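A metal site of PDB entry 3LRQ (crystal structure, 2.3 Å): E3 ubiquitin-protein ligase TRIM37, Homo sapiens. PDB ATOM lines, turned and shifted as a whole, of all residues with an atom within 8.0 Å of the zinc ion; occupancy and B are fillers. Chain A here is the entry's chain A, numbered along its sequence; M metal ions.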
ATOM      1  N   ARG A  24     -12.104  -6.218  -5.422  1.00  0.00           N
ATOM      2  CA  ARG A  24     -13.165  -5.915  -4.494  1.00  0.00           C
ATOM      3  C   ARG A  24     -12.563  -5.916  -3.103  1.00  0.00           C
ATOM      4  O   ARG A  24     -11.573  -6.597  -2.837  1.00  0.00           O
ATOM      5  CB  ARG A  24     -14.303  -6.925  -4.624  1.00  0.00           C
ATOM      6  CG  ARG A  24     -15.234  -6.626  -5.805  1.00  0.00           C
ATOM      7  CD  ARG A  24     -16.436  -7.581  -5.863  1.00  0.00           C
ATOM      8  NE  ARG A  24     -17.474  -7.150  -6.804  1.00  0.00           N
ATOM      9  CZ  ARG A  24     -17.541  -7.531  -8.082  1.00  0.00           C
ATOM     10  NH1 ARG A  24     -16.631  -8.344  -8.598  1.00  0.00           N
ATOM     11  NH2 ARG A  24     -18.526  -7.086  -8.861  1.00  0.00           N
ATOM     12  N   CYS A  25     -13.127  -5.101  -2.229  1.00  0.00           N
ATOM     13  CA  CYS A  25     -12.647  -4.957  -0.863  1.00  0.00           C
ATOM     14  C   CYS A  25     -12.882  -6.244  -0.050  1.00  0.00           C
ATOM     15  O   CYS A  25     -14.015  -6.735   0.056  1.00  0.00           O
ATOM     16  CB  CYS A  25     -13.388  -3.797  -0.211  1.00  0.00           C
ATOM     17  SG  CYS A  25     -12.905  -3.452   1.516  1.00  0.00           S
ATOM     18  N   PHE A  26     -11.828  -6.793   0.556  1.00  0.00           N
ATOM     19  CA  PHE A  26     -11.984  -8.011   1.340  1.00  0.00           C
ATOM     20  C   PHE A  26     -13.011  -7.742   2.428  1.00  0.00           C
ATOM     21  O   PHE A  26     -13.825  -8.597   2.765  1.00  0.00           O
ATOM     22  CB  PHE A  26     -10.658  -8.407   1.985  1.00  0.00           C
ATOM     23  CG  PHE A  26     -10.702  -9.687   2.762  1.00  0.00           C
ATOM     24  CD1 PHE A  26     -10.557 -10.921   2.124  1.00  0.00           C
ATOM     25  CD2 PHE A  26     -10.881  -9.674   4.149  1.00  0.00           C
ATOM     26  CE1 PHE A  26     -10.605 -12.127   2.835  1.00  0.00           C
ATOM     27  CE2 PHE A  26     -10.901 -10.870   4.880  1.00  0.00           C
ATOM     28  CZ  PHE A  26     -10.768 -12.099   4.227  1.00  0.00           C
ATOM     29  N   ILE A  27     -12.973  -6.538   2.985  1.00  0.00           N
ATOM     30  CA  ILE A  27     -13.860  -6.261   4.109  1.00  0.00           C
ATOM     31  C   ILE A  27     -15.330  -6.050   3.749  1.00  0.00           C
ATOM     32  O   ILE A  27     -16.199  -6.609   4.392  1.00  0.00           O
ATOM     33  CB  ILE A  27     -13.347  -5.108   4.966  1.00  0.00           C
ATOM     34  CG1 ILE A  27     -12.014  -5.510   5.591  1.00  0.00           C
ATOM     35  CG2 ILE A  27     -14.385  -4.743   6.043  1.00  0.00           C
ATOM     36  CD1 ILE A  27     -11.279  -4.347   6.213  1.00  0.00           C
ATOM     37  N   CYS A  28     -15.606  -5.231   2.735  1.00  0.00           N
ATOM     38  CA  CYS A  28     -17.004  -4.892   2.439  1.00  0.00           C
ATOM     39  C   CYS A  28     -17.472  -5.526   1.140  1.00  0.00           C
ATOM     40  O   CYS A  28     -18.615  -5.383   0.754  1.00  0.00           O
ATOM     41  CB  CYS A  28     -17.186  -3.353   2.391  1.00  0.00           C
ATOM     42  SG  CYS A  28     -16.641  -2.591   0.825  1.00  0.00           S
ATOM     43  N   MET A  29     -16.547  -6.186   0.434  1.00  0.00           N
ATOM     44  CA  MET A  29     -16.832  -6.837  -0.834  1.00  0.00           C
ATOM     45  C   MET A  29     -17.455  -5.889  -1.879  1.00  0.00           C
ATOM     46  O   MET A  29     -17.986  -6.349  -2.879  1.00  0.00           O
ATOM     47  CB  MET A  29     -17.621  -8.159  -0.646  1.00  0.00           C
ATOM     48  CG  MET A  29     -16.747  -9.353  -0.025  1.00  0.00           C
ATOM     49  SD  MET A  29     -14.903  -9.641  -0.887  1.00  0.00           S
ATOM     50  CE  MET A  29     -15.461  -9.802  -2.757  1.00  0.00           C
ATOM     51  N   GLU A  30     -17.373  -4.587  -1.647  1.00  0.00           N
ATOM     52  CA  GLU A  30     -17.707  -3.626  -2.700  1.00  0.00           C
ATOM     53  C   GLU A  30     -16.491  -3.319  -3.566  1.00  0.00           C
ATOM     54  O   GLU A  30     -15.353  -3.719  -3.249  1.00  0.00           O
ATOM     55  CB  GLU A  30     -18.267  -2.332  -2.113  1.00  0.00           C
ATOM     56  CG  GLU A  30     -19.635  -2.499  -1.436  1.00  0.00           C
ATOM     57  CD  GLU A  30     -20.610  -3.326  -2.257  1.00  0.00           C
ATOM     58  OE1 GLU A  30     -20.547  -3.281  -3.502  1.00  0.00           O
ATOM     59  OE2 GLU A  30     -21.445  -4.034  -1.653  1.00  0.00           O
ATOM     60  N   LYS A  31     -16.716  -2.643  -4.684  1.00  0.00           N
ATOM     61  CA  LYS A  31     -15.575  -2.290  -5.513  1.00  0.00           C
ATOM     62  C   LYS A  31     -14.736  -1.300  -4.713  1.00  0.00           C
ATOM     63  O   LYS A  31     -15.239  -0.558  -3.887  1.00  0.00           O
ATOM     64  CB  LYS A  31     -15.983  -1.765  -6.905  1.00  0.00           C
ATOM     65  CG  LYS A  31     -16.571  -0.381  -6.935  1.00  0.00           C
ATOM     66  CD  LYS A  31     -15.984   0.405  -8.112  1.00  0.00           C
ATOM     67  CE  LYS A  31     -16.916   1.510  -8.594  1.00  0.00           C
ATOM     68  NZ  LYS A  31     -18.063   0.966  -9.379  1.00  0.00           N
ATOM     69  N   LEU A  32     -13.431  -1.342  -4.937  1.00  0.00           N
ATOM     70  CA  LEU A  32     -12.503  -0.656  -4.070  1.00  0.00           C
ATOM     71  C   LEU A  32     -12.613   0.854  -4.214  1.00  0.00           C
ATOM     72  O   LEU A  32     -12.678   1.363  -5.331  1.00  0.00           O
ATOM     73  CB  LEU A  32     -11.068  -1.111  -4.379  1.00  0.00           C
ATOM     74  CG  LEU A  32     -10.665  -2.510  -3.892  1.00  0.00           C
ATOM     75  CD1 LEU A  32      -9.510  -3.061  -4.738  1.00  0.00           C
ATOM     76  CD2 LEU A  32     -10.273  -2.457  -2.429  1.00  0.00           C
ATOM     77  N   ARG A  33     -12.654   1.552  -3.089  1.00  0.00           N
ATOM     78  CA  ARG A  33     -12.458   2.998  -3.038  1.00  0.00           C
ATOM     79  C   ARG A  33     -11.181   3.334  -2.255  1.00  0.00           C
ATOM     80  O   ARG A  33     -11.041   2.987  -1.079  1.00  0.00           O
ATOM     81  CB  ARG A  33     -13.679   3.695  -2.423  1.00  0.00           C
ATOM     82  CG  ARG A  33     -13.386   5.099  -1.904  1.00  0.00           C
ATOM     83  CD  ARG A  33     -14.522   6.082  -2.136  1.00  0.00           C
ATOM     84  NE  ARG A  33     -14.288   7.365  -1.460  1.00  0.00           N
ATOM     85  CZ  ARG A  33     -14.958   8.480  -1.713  1.00  0.00           C
ATOM     86  NH1 ARG A  33     -15.910   8.489  -2.637  1.00  0.00           N
ATOM     87  NH2 ARG A  33     -14.681   9.591  -1.037  1.00  0.00           N
ATOM     88  N   LEU A  44      -6.541  -6.589  -0.758  1.00  0.00           N
ATOM     89  CA  LEU A  44      -6.900  -5.187  -0.932  1.00  0.00           C
ATOM     90  C   LEU A  44      -8.170  -4.843  -0.139  1.00  0.00           C
ATOM     91  O   LEU A  44      -9.106  -5.635  -0.110  1.00  0.00           O
ATOM     92  CB  LEU A  44      -7.125  -4.888  -2.416  1.00  0.00           C
ATOM     93  CG  LEU A  44      -5.928  -4.972  -3.384  1.00  0.00           C
ATOM     94  CD1 LEU A  44      -6.251  -5.834  -4.583  1.00  0.00           C
ATOM     95  CD2 LEU A  44      -5.440  -3.575  -3.846  1.00  0.00           C
ATOM     96  N   CYS A  45      -8.177  -3.654   0.477  1.00  0.00           N
ATOM     97  CA  CYS A  45      -9.350  -3.059   1.126  1.00  0.00           C
ATOM     98  C   CYS A  45      -9.496  -1.561   0.820  1.00  0.00           C
ATOM     99  O   CYS A  45      -8.488  -0.855   0.594  1.00  0.00           O
ATOM    100  CB  CYS A  45      -9.252  -3.171   2.643  1.00  0.00           C
ATOM    101  SG  CYS A  45      -9.056  -4.816   3.288  1.00  0.00           S
ATOM    102  N   CYS A  46     -10.734  -1.065   0.832  1.00  0.00           N
ATOM    103  CA  CYS A  46     -10.956   0.370   0.797  1.00  0.00           C
ATOM    104  C   CYS A  46     -10.205   1.007   1.968  1.00  0.00           C
ATOM    105  O   CYS A  46     -10.101   0.414   3.039  1.00  0.00           O
ATOM    106  CB  CYS A  46     -12.442   0.705   0.921  1.00  0.00           C
ATOM    107  SG  CYS A  46     -13.562  -0.208  -0.226  1.00  0.00           S
ATOM    108  N   PHE A  47      -9.687   2.211   1.765  1.00  0.00           N
ATOM    109  CA  PHE A  47      -9.010   2.879   2.861  1.00  0.00           C
ATOM    110  C   PHE A  47      -9.921   2.975   4.078  1.00  0.00           C
ATOM    111  O   PHE A  47      -9.506   2.711   5.203  1.00  0.00           O
ATOM    112  CB  PHE A  47      -8.558   4.281   2.470  1.00  0.00           C
ATOM    113  CG  PHE A  47      -8.112   5.096   3.647  1.00  0.00           C
ATOM    114  CD1 PHE A  47      -6.858   4.912   4.194  1.00  0.00           C
ATOM    115  CD2 PHE A  47      -8.980   5.998   4.237  1.00  0.00           C
ATOM    116  CE1 PHE A  47      -6.445   5.645   5.303  1.00  0.00           C
ATOM    117  CE2 PHE A  47      -8.574   6.746   5.344  1.00  0.00           C
ATOM    118  CZ  PHE A  47      -7.297   6.558   5.871  1.00  0.00           C
ATOM    119  N   SER A  48     -11.158   3.386   3.873  1.00  0.00           N
ATOM    120  CA  SER A  48     -12.032   3.645   5.006  1.00  0.00           C
ATOM    121  C   SER A  48     -12.325   2.358   5.733  1.00  0.00           C
ATOM    122  O   SER A  48     -12.558   2.368   6.949  1.00  0.00           O
ATOM    123  CB  SER A  48     -13.356   4.237   4.572  1.00  0.00           C
ATOM    124  OG  SER A  48     -13.185   5.488   3.934  1.00  0.00           O
ATOM    125  N   CYS A  49     -12.346   1.238   5.002  1.00  0.00           N
ATOM    126  CA  CYS A  49     -12.766  -0.033   5.584  1.00  0.00           C
ATOM    127  C   CYS A  49     -11.650  -0.540   6.435  1.00  0.00           C
ATOM    128  O   CYS A  49     -11.853  -0.839   7.603  1.00  0.00           O
ATOM    129  CB  CYS A  49     -13.109  -1.066   4.491  1.00  0.00           C
ATOM    130  SG  CYS A  49     -14.656  -0.690   3.634  1.00  0.00           S
ATOM    131  N   ILE A  50     -10.447  -0.592   5.862  1.00  0.00           N
ATOM    132  CA  ILE A  50      -9.330  -1.126   6.595  1.00  0.00           C
ATOM    133  C   ILE A  50      -9.017  -0.169   7.768  1.00  0.00           C
ATOM    134  O   ILE A  50      -8.617  -0.612   8.857  1.00  0.00           O
ATOM    135  CB  ILE A  50      -8.118  -1.372   5.682  1.00  0.00           C
ATOM    136  CG1 ILE A  50      -6.992  -2.127   6.428  1.00  0.00           C
ATOM    137  CG2 ILE A  50      -7.598  -0.022   5.069  1.00  0.00           C
ATOM    138  CD1 ILE A  50      -7.434  -3.278   7.323  1.00  0.00           C
ATOM    139  N   ARG A  52     -11.127   1.707   9.566  1.00  0.00           N
ATOM    140  CA  ARG A  52     -12.103   1.342  10.576  1.00  0.00           C
ATOM    141  C   ARG A  52     -11.753  -0.033  11.209  1.00  0.00           C
ATOM    142  O   ARG A  52     -11.855  -0.200  12.405  1.00  0.00           O
ATOM    143  CB  ARG A  52     -13.496   1.319   9.953  1.00  0.00           C
ATOM    144  CG  ARG A  52     -14.619   1.021  10.947  1.00  0.00           C
ATOM    145  CD  ARG A  52     -15.969   0.921  10.263  1.00  0.00           C
ATOM    146  NE  ARG A  52     -16.322   2.185   9.636  1.00  0.00           N
ATOM    147  CZ  ARG A  52     -16.348   2.383   8.314  1.00  0.00           C
ATOM    148  NH1 ARG A  52     -16.086   1.371   7.478  1.00  0.00           N
ATOM    149  NH2 ARG A  52     -16.668   3.576   7.824  1.00  0.00           N
HETATM  150 ZN    ZN M   1     -14.510  -1.672   1.483  1.00  0.00          ZN
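SG of Cys 25 sits close to N of Ile 27. N of Cys 25 lies within hydrogen-bond range of O of Glu 30, at 2.8 Å. N of Glu 30 lies close to SG of Cys 28, 3.3 Å away. The side-chain sulfur (SG) of Cys 46 lies close to the backbone NH (N) of Arg 33 (3.5 Å).
Of the 18 residues printed, 4 come within 4 Å of the zinc ion.
The side-chain sulfur (SG) of Cys 49 is bound to the zinc ion, at 2.4 Å. SG of Cys 25 binds the zinc ion, 2.4 Å away. The zinc ion is bound by SG of Cys 28 (2.4 Å). The side-chain sulfur (SG) of Cys 46 is bound to the zinc ion, 2.4 Å away. The zinc ion has four donor atoms within binding distance.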
